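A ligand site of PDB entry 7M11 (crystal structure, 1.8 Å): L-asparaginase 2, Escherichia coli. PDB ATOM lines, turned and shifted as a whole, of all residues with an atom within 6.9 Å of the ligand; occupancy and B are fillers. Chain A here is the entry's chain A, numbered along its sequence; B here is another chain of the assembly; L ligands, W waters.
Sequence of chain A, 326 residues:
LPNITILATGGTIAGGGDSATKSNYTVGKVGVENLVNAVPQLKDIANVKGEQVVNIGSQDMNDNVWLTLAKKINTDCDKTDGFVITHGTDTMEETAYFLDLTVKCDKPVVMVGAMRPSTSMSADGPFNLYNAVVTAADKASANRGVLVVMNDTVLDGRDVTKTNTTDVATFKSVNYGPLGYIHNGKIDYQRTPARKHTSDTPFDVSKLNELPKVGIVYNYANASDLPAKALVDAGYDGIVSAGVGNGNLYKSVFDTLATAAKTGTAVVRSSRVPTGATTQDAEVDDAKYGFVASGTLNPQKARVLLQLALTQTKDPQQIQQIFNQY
A nitrogen (N1) of the ligand sits at hydrogen-bond distance from the side-chain amide oxygen (OE1) of Gln 59 (2.8 Å).
OG of Ser 58 is in hydrogen-bond range of O1 of the ligand, 2.4 Å away.
The side-chain carboxylate (OD1) of Asp 90 lies within salt-bridge range of a nitrogen (N1) of the ligand.
The backbone NH (N) of Thr 89 is in hydrogen-bond range of an oxygen (O3) of the ligand.
An oxygen (O4) of the ligand sits at hydrogen-bond distance from the backbone NH (N) of Ser 58 (2.7 Å).
The backbone NH (N) of Thr 12 is in hydrogen-bond range of an oxygen (O3) of the ligand (2.9 Å).
N of Asp 90 lies within hydrogen-bond range of O1 of the ligand (2.8 Å).
An oxygen (O2) of the ligand is in hydrogen-bond range of the side-chain hydroxyl of Thr 89.
ND2 of Asn 248 of chain B sits close to N1 of the ligand, 3.5 Å away.
The side-chain hydroxyl (OG1) of Thr 12 lies close to an oxygen (O3) of the ligand.
A nitrogen (N1) of the ligand lies within salt-bridge range of the side-chain carboxylate (OE1) of Glu 283 of chain B (2.5 Å).
The side-chain hydroxyl (OG) of Ser 58 is in hydrogen-bond range of the backbone NH (N) of Asp 90, at 3.2 Å.
The side-chain hydroxyl (OH) of Tyr 25 is in hydrogen-bond range of the side-chain carboxylate (OE1) of Glu 283 of chain B, at 3.3 Å.
SD of Met 115 lies within hydrogen-bond range of OG1 of Thr 89.
The side-chain hydroxyl (OG) of Ser 58 lies close to the backbone carbonyl oxygen (O) of Gly 88.
O of Ser 58 sits at hydrogen-bond distance from OG1 of Thr 91.
The side-chain carboxylate (OD1) of Asp 90 sits at hydrogen-bond distance from the side-chain amide nitrogen (ND2) of Asn 248 of chain B (2.6 Å).
NZ of Lys 162 is in hydrogen-bond range of OG1 of Thr 89, 2.5 Å away.
The side-chain hydroxyl of Tyr 25 is in hydrogen-bond range of the side-chain hydroxyl of Thr 12 (2.7 Å).
O of Ala 114 lies close to O2 of the ligand (3.2 Å).
Residues that only touch the ligand: Gly 11 (3.4 Å), Tyr 25 (3.7 Å), Gly 57 (3.5 Å) and Gly 88 (3.2 Å).
Of the 29 residues printed, 12 come within 4 Å of the ligand.
Water W2 lies within hydrogen-bond range of O2 of the ligand (2.7 Å), OH of Tyr 25 (3.0 Å) and O of Met 115 (3.1 Å).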
ATOM      1  N   GLY A  10      32.265  20.969   5.787  1.00  0.00           N
ATOM      2  CA  GLY A  10      30.938  20.498   6.122  1.00  0.00           C
ATOM      3  C   GLY A  10      30.956  19.061   6.622  1.00  0.00           C
ATOM      4  O   GLY A  10      31.792  18.687   7.472  1.00  0.00           O
ATOM      5  N   GLY A  11      30.016  18.262   6.115  1.00  0.00           N
ATOM      6  CA  GLY A  11      29.912  16.861   6.484  1.00  0.00           C
ATOM      7  C   GLY A  11      29.056  16.626   7.707  1.00  0.00           C
ATOM      8  O   GLY A  11      28.608  17.535   8.399  1.00  0.00           O
ATOM      9  N   THR A  12      28.819  15.329   7.967  1.00  0.00           N
ATOM     10  CA  THR A  12      28.058  14.918   9.151  1.00  0.00           C
ATOM     11  C   THR A  12      28.727  15.363  10.429  1.00  0.00           C
ATOM     12  O   THR A  12      28.038  15.639  11.428  1.00  0.00           O
ATOM     13  CB  THR A  12      27.872  13.401   9.156  1.00  0.00           C
ATOM     14  OG1 THR A  12      26.970  13.036   8.111  1.00  0.00           O
ATOM     15  CG2 THR A  12      27.360  12.871  10.500  1.00  0.00           C
ATOM     16  N   ILE A  13      30.067  15.465  10.441  1.00  0.00           N
ATOM     17  CA  ILE A  13      30.748  15.979  11.633  1.00  0.00           C
ATOM     18  C   ILE A  13      30.164  17.322  12.019  1.00  0.00           C
ATOM     19  O   ILE A  13      30.045  17.631  13.218  1.00  0.00           O
ATOM     20  CB  ILE A  13      32.286  16.036  11.404  1.00  0.00           C
ATOM     21  CG1 ILE A  13      33.021  16.397  12.699  1.00  0.00           C
ATOM     22  CG2 ILE A  13      32.683  17.022  10.282  1.00  0.00           C
ATOM     23  CD1 ILE A  13      34.507  16.016  12.659  1.00  0.00           C
ATOM     24  N   ALA A  14      29.716  18.107  11.032  1.00  0.00           N
ATOM     25  CA  ALA A  14      29.092  19.397  11.253  1.00  0.00           C
ATOM     26  C   ALA A  14      27.598  19.382  10.991  1.00  0.00           C
ATOM     27  O   ALA A  14      26.928  20.377  11.283  1.00  0.00           O
ATOM     28  CB  ALA A  14      29.755  20.459  10.359  1.00  0.00           C
ATOM     29  N   TYR A  25      19.072  12.907   9.224  1.00  0.00           N
ATOM     30  CA  TYR A  25      19.757  14.135   9.624  1.00  0.00           C
ATOM     31  C   TYR A  25      20.175  14.926   8.397  1.00  0.00           C
ATOM     32  O   TYR A  25      20.315  14.380   7.292  1.00  0.00           O
ATOM     33  CB  TYR A  25      20.996  13.824  10.480  1.00  0.00           C
ATOM     34  CG  TYR A  25      22.123  13.106   9.736  1.00  0.00           C
ATOM     35  CD1 TYR A  25      23.106  13.813   9.066  1.00  0.00           C
ATOM     36  CD2 TYR A  25      22.194  11.716   9.743  1.00  0.00           C
ATOM     37  CE1 TYR A  25      24.123  13.150   8.400  1.00  0.00           C
ATOM     38  CE2 TYR A  25      23.215  11.049   9.086  1.00  0.00           C
ATOM     39  CZ  TYR A  25      24.181  11.762   8.413  1.00  0.00           C
ATOM     40  OH  TYR A  25      25.193  11.076   7.765  1.00  0.00           O
ATOM     41  N   GLY A  28      26.003  19.352   6.648  1.00  0.00           N
ATOM     42  CA  GLY A  28      26.855  20.474   6.933  1.00  0.00           C
ATOM     43  C   GLY A  28      26.159  21.749   7.321  1.00  0.00           C
ATOM     44  O   GLY A  28      25.791  22.559   6.444  1.00  0.00           O
ATOM     45  N   ILE A  56      28.977  22.010   3.150  1.00  0.00           N
ATOM     46  CA  ILE A  56      28.130  21.170   2.308  1.00  0.00           C
ATOM     47  C   ILE A  56      28.283  19.720   2.743  1.00  0.00           C
ATOM     48  O   ILE A  56      29.246  19.347   3.412  1.00  0.00           O
ATOM     49  CB  ILE A  56      28.455  21.221   0.808  1.00  0.00           C
ATOM     50  CG1 ILE A  56      29.927  20.871   0.527  1.00  0.00           C
ATOM     51  CG2 ILE A  56      28.152  22.622   0.263  1.00  0.00           C
ATOM     52  CD1 ILE A  56      30.301  20.920  -0.970  1.00  0.00           C
ATOM     53  N   GLY A  57      27.320  18.900   2.338  1.00  0.00           N
ATOM     54  CA  GLY A  57      27.526  17.453   2.377  1.00  0.00           C
ATOM     55  C   GLY A  57      28.534  17.037   1.318  1.00  0.00           C
ATOM     56  O   GLY A  57      28.443  17.453   0.152  1.00  0.00           O
ATOM     57  N   SER A  58      29.496  16.206   1.721  1.00  0.00           N
ATOM     58  CA  SER A  58      30.547  15.826   0.788  1.00  0.00           C
ATOM     59  C   SER A  58      30.031  14.984  -0.379  1.00  0.00           C
ATOM     60  O   SER A  58      30.787  14.738  -1.318  1.00  0.00           O
ATOM     61  CB  SER A  58      31.667  15.070   1.514  1.00  0.00           C
ATOM     62  OG  SER A  58      31.294  13.721   1.768  1.00  0.00           O
ATOM     63  N   GLN A  59      28.761  14.561  -0.351  1.00  0.00           N
ATOM     64  CA  GLN A  59      28.191  13.992  -1.567  1.00  0.00           C
ATOM     65  C   GLN A  59      28.089  15.048  -2.667  1.00  0.00           C
ATOM     66  O   GLN A  59      27.895  14.702  -3.834  1.00  0.00           O
ATOM     67  CB  GLN A  59      26.785  13.396  -1.334  1.00  0.00           C
ATOM     68  CG  GLN A  59      25.691  14.353  -0.813  1.00  0.00           C
ATOM     69  CD  GLN A  59      25.588  14.334   0.699  1.00  0.00           C
ATOM     70  OE1 GLN A  59      26.585  14.416   1.412  1.00  0.00           O
ATOM     71  NE2 GLN A  59      24.377  14.146   1.199  1.00  0.00           N
ATOM     72  N   ASP A  60      28.209  16.315  -2.305  1.00  0.00           N
ATOM     73  CA  ASP A  60      28.176  17.409  -3.257  1.00  0.00           C
ATOM     74  C   ASP A  60      29.554  18.014  -3.487  1.00  0.00           C
ATOM     75  O   ASP A  60      29.644  19.109  -4.044  1.00  0.00           O
ATOM     76  CB  ASP A  60      27.207  18.482  -2.775  1.00  0.00           C
ATOM     77  CG  ASP A  60      25.771  18.038  -2.854  1.00  0.00           C
ATOM     78  OD1 ASP A  60      25.475  17.064  -3.599  1.00  0.00           O
ATOM     79  OD2 ASP A  60      24.934  18.653  -2.149  1.00  0.00           O
ATOM     80  N   HIS A  87      35.465  17.415   6.998  1.00  0.00           N
ATOM     81  CA  HIS A  87      34.958  16.988   5.697  1.00  0.00           C
ATOM     82  C   HIS A  87      33.920  15.901   5.900  1.00  0.00           C
ATOM     83  O   HIS A  87      33.980  15.152   6.889  1.00  0.00           O
ATOM     84  CB  HIS A  87      36.126  16.476   4.837  1.00  0.00           C
ATOM     85  CG  HIS A  87      35.811  16.286   3.384  1.00  0.00           C
ATOM     86  ND1 HIS A  87      35.176  15.160   2.893  1.00  0.00           N
ATOM     87  CD2 HIS A  87      36.138  17.021   2.287  1.00  0.00           C
ATOM     88  CE1 HIS A  87      35.088  15.236   1.578  1.00  0.00           C
ATOM     89  NE2 HIS A  87      35.680  16.346   1.187  1.00  0.00           N
ATOM     90  N   GLY A  88      32.994  15.813   4.960  1.00  0.00           N
ATOM     91  CA  GLY A  88      32.092  14.670   4.930  1.00  0.00           C
ATOM     92  C   GLY A  88      32.825  13.381   4.613  1.00  0.00           C
ATOM     93  O   GLY A  88      33.835  13.371   3.905  1.00  0.00           O
ATOM     94  N   THR A  89      32.328  12.281   5.191  1.00  0.00           N
ATOM     95  CA  THR A  89      32.960  10.980   4.975  1.00  0.00           C
ATOM     96  C   THR A  89      32.660  10.375   3.602  1.00  0.00           C
ATOM     97  O   THR A  89      33.430   9.529   3.147  1.00  0.00           O
ATOM     98  CB  THR A  89      32.544   9.974   6.066  1.00  0.00           C
ATOM     99  OG1 THR A  89      31.204   9.529   5.828  1.00  0.00           O
ATOM    100  CG2 THR A  89      32.674  10.577   7.470  1.00  0.00           C
ATOM    101  N   ASP A  90      31.593  10.805   2.933  1.00  0.00           N
ATOM    102  CA  ASP A  90      31.184  10.167   1.671  1.00  0.00           C
ATOM    103  C   ASP A  90      32.283  10.233   0.607  1.00  0.00           C
ATOM    104  O   ASP A  90      32.563   9.233  -0.067  1.00  0.00           O
ATOM    105  CB  ASP A  90      29.887  10.800   1.155  1.00  0.00           C
ATOM    106  CG  ASP A  90      28.631  10.360   1.946  1.00  0.00           C
ATOM    107  OD1 ASP A  90      27.533  10.816   1.582  1.00  0.00           O
ATOM    108  OD2 ASP A  90      28.703   9.614   2.943  1.00  0.00           O
ATOM    109  N   THR A  91      32.906  11.402   0.408  1.00  0.00           N
ATOM    110  CA  THR A  91      33.955  11.530  -0.609  1.00  0.00           C
ATOM    111  C   THR A  91      35.279  11.941   0.001  1.00  0.00           C
ATOM    112  O   THR A  91      36.156  12.476  -0.697  1.00  0.00           O
ATOM    113  CB  THR A  91      33.581  12.530  -1.698  1.00  0.00           C
ATOM    114  OG1 THR A  91      33.350  13.818  -1.098  1.00  0.00           O
ATOM    115  CG2 THR A  91      32.335  12.087  -2.468  1.00  0.00           C
ATOM    116  N   MET A  92      35.449  11.741   1.306  1.00  0.00           N
ATOM    117  CA  MET A  92      36.683  12.188   1.926  1.00  0.00           C
ATOM    118  C   MET A  92      37.884  11.478   1.322  1.00  0.00           C
ATOM    119  O   MET A  92      38.968  12.058   1.251  1.00  0.00           O
ATOM    120  CB  MET A  92      36.619  11.960   3.435  1.00  0.00           C
ATOM    121  CG  MET A  92      37.373  13.019   4.227  1.00  0.00           C
ATOM    122  SD  MET A  92      37.999  12.544   5.835  1.00  0.00           S
ATOM    123  CE  MET A  92      36.524  12.011   6.674  1.00  0.00           C
ATOM    124  N   GLY A 113      36.437  13.344   9.648  1.00  0.00           N
ATOM    125  CA  GLY A 113      34.994  13.445   9.608  1.00  0.00           C
ATOM    126  C   GLY A 113      34.317  12.671  10.728  1.00  0.00           C
ATOM    127  O   GLY A 113      34.965  12.259  11.695  1.00  0.00           O
ATOM    128  N   ALA A 114      33.008  12.460  10.619  1.00  0.00           N
ATOM    129  CA  ALA A 114      32.293  11.740  11.658  1.00  0.00           C
ATOM    130  C   ALA A 114      31.121  11.005  11.025  1.00  0.00           C
ATOM    131  O   ALA A 114      30.442  11.563  10.153  1.00  0.00           O
ATOM    132  CB  ALA A 114      31.815  12.680  12.777  1.00  0.00           C
ATOM    133  N   MET A 115      30.892   9.779  11.455  1.00  0.00           N
ATOM    134  CA  MET A 115      29.871   8.939  10.846  1.00  0.00           C
ATOM    135  C   MET A 115      28.518   9.084  11.545  1.00  0.00           C
ATOM    136  O   MET A 115      27.487   8.692  10.972  1.00  0.00           O
ATOM    137  CB  MET A 115      30.323   7.473  10.875  1.00  0.00           C
ATOM    138  CG  MET A 115      31.440   7.254   9.872  1.00  0.00           C
ATOM    139  SD  MET A 115      30.854   7.253   8.186  1.00  0.00           S
ATOM    140  CE  MET A 115      29.831   5.775   8.101  1.00  0.00           C
ATOM    141  N   ARG A 116      28.495   9.646  12.742  1.00  0.00           N
ATOM    142  CA  ARG A 116      27.317   9.947  13.526  1.00  0.00           C
ATOM    143  C   ARG A 116      27.148  11.449  13.697  1.00  0.00           C
ATOM    144  O   ARG A 116      28.135  12.184  13.761  1.00  0.00           O
ATOM    145  CB  ARG A 116      27.433   9.268  14.899  1.00  0.00           C
ATOM    146  CG  ARG A 116      27.467   7.762  14.802  1.00  0.00           C
ATOM    147  CD  ARG A 116      27.961   7.157  16.105  1.00  0.00           C
ATOM    148  NE  ARG A 116      27.779   5.709  16.149  1.00  0.00           N
ATOM    149  CZ  ARG A 116      28.202   4.931  17.147  1.00  0.00           C
ATOM    150  NH1 ARG A 116      28.859   5.445  18.182  1.00  0.00           N
ATOM    151  NH2 ARG A 116      27.980   3.630  17.091  1.00  0.00           N
ATOM    152  N   LYS A 162      36.369   4.321   2.104  1.00  0.00           N
ATOM    153  CA  LYS A 162      35.196   4.063   2.956  1.00  0.00           C
ATOM    154  C   LYS A 162      34.646   2.653   2.677  1.00  0.00           C
ATOM    155  O   LYS A 162      34.139   2.400   1.577  1.00  0.00           O
ATOM    156  CB  LYS A 162      34.119   5.124   2.715  1.00  0.00           C
ATOM    157  CG  LYS A 162      32.928   5.074   3.674  1.00  0.00           C
ATOM    158  CD  LYS A 162      32.012   6.313   3.507  1.00  0.00           C
ATOM    159  CE  LYS A 162      30.786   6.206   4.421  1.00  0.00           C
ATOM    160  NZ  LYS A 162      30.183   7.552   4.781  1.00  0.00           N
ATOM    161  N   THR A 165      28.954   1.397   5.050  1.00  0.00           N
ATOM    162  CA  THR A 165      28.063   2.531   4.878  1.00  0.00           C
ATOM    163  C   THR A 165      27.794   3.271   6.185  1.00  0.00           C
ATOM    164  O   THR A 165      27.564   4.483   6.157  1.00  0.00           O
ATOM    165  CB  THR A 165      26.748   2.081   4.255  1.00  0.00           C
ATOM    166  OG1 THR A 165      26.152   1.110   5.104  1.00  0.00           O
ATOM    167  CG2 THR A 165      26.949   1.482   2.858  1.00  0.00           C
ATOM    168  N   VAL B 244      27.351   7.353  -2.823  1.00  0.00           N
ATOM    169  CA  VAL B 244      28.464   7.495  -1.906  1.00  0.00           C
ATOM    170  C   VAL B 244      27.937   7.313  -0.496  1.00  0.00           C
ATOM    171  O   VAL B 244      26.783   7.670  -0.203  1.00  0.00           O
ATOM    172  CB  VAL B 244      29.194   8.841  -2.110  1.00  0.00           C
ATOM    173  CG1 VAL B 244      29.861   8.887  -3.467  1.00  0.00           C
ATOM    174  CG2 VAL B 244      28.233  10.022  -1.988  1.00  0.00           C
ATOM    175  N   GLY B 245      28.750   6.727   0.371  1.00  0.00           N
ATOM    176  CA  GLY B 245      28.323   6.568   1.760  1.00  0.00           C
ATOM    177  C   GLY B 245      27.073   5.722   1.866  1.00  0.00           C
ATOM    178  O   GLY B 245      26.911   4.709   1.192  1.00  0.00           O
ATOM    179  N   ASN B 246      26.137   6.176   2.709  1.00  0.00           N
ATOM    180  CA  ASN B 246      24.859   5.501   2.883  1.00  0.00           C
ATOM    181  C   ASN B 246      23.889   5.919   1.765  1.00  0.00           C
ATOM    182  O   ASN B 246      22.883   6.598   1.989  1.00  0.00           O
ATOM    183  CB  ASN B 246      24.278   5.793   4.253  1.00  0.00           C
ATOM    184  CG  ASN B 246      23.041   4.981   4.562  1.00  0.00           C
ATOM    185  OD1 ASN B 246      22.646   4.086   3.799  1.00  0.00           O
ATOM    186  ND2 ASN B 246      22.422   5.267   5.692  1.00  0.00           N
ATOM    187  N   ASN B 248      24.120   8.029  -0.779  1.00  0.00           N
ATOM    188  CA  ASN B 248      23.919   9.435  -1.119  1.00  0.00           C
ATOM    189  C   ASN B 248      24.288   9.749  -2.566  1.00  0.00           C
ATOM    190  O   ASN B 248      25.009   9.003  -3.240  1.00  0.00           O
ATOM    191  CB  ASN B 248      24.717  10.353  -0.183  1.00  0.00           C
ATOM    192  CG  ASN B 248      24.177  10.311   1.226  1.00  0.00           C
ATOM    193  OD1 ASN B 248      22.956  10.382   1.412  1.00  0.00           O
ATOM    194  ND2 ASN B 248      25.053  10.161   2.209  1.00  0.00           N
ATOM    195  N   GLU B 283      19.657  10.239   4.961  1.00  0.00           N
ATOM    196  CA  GLU B 283      19.813  11.598   4.451  1.00  0.00           C
ATOM    197  C   GLU B 283      18.823  11.938   3.352  1.00  0.00           C
ATOM    198  O   GLU B 283      18.530  13.108   3.139  1.00  0.00           O
ATOM    199  CB  GLU B 283      21.250  11.825   3.952  1.00  0.00           C
ATOM    200  CG  GLU B 283      22.172  12.389   5.033  1.00  0.00           C
ATOM    201  CD  GLU B 283      23.562  12.790   4.522  1.00  0.00           C
ATOM    202  OE1 GLU B 283      24.510  12.003   4.710  1.00  0.00           O
ATOM    203  OE2 GLU B 283      23.727  13.893   3.950  1.00  0.00           O
HETATM  204  N1  LIG L   1      26.665  12.853   3.676  1.00  0.00           N
HETATM  205  C1  LIG L   1      27.698  13.008   4.691  1.00  0.00           C
HETATM  206  C2  LIG L   1      28.909  13.572   3.973  1.00  0.00           C
HETATM  207  O1  LIG L   1      29.700  12.854   3.368  1.00  0.00           O
HETATM  208  C3  LIG L   1      27.993  11.682   5.403  1.00  0.00           C
HETATM  209  C4  LIG L   1      29.041  11.804   6.504  1.00  0.00           C
HETATM  210  O2  LIG L   1      29.223  10.830   7.276  1.00  0.00           O
HETATM  211  O3  LIG L   1      29.634  12.900   6.672  1.00  0.00           O
HETATM  212  O4  LIG L   1      29.055  14.795   3.960  1.00  0.00           O
HETATM  213  O   HOH W   1      31.735  13.970   8.553  1.00  0.00           O
HETATM  214  O   HOH W   2      27.277   8.979   7.851  1.00  0.00           O
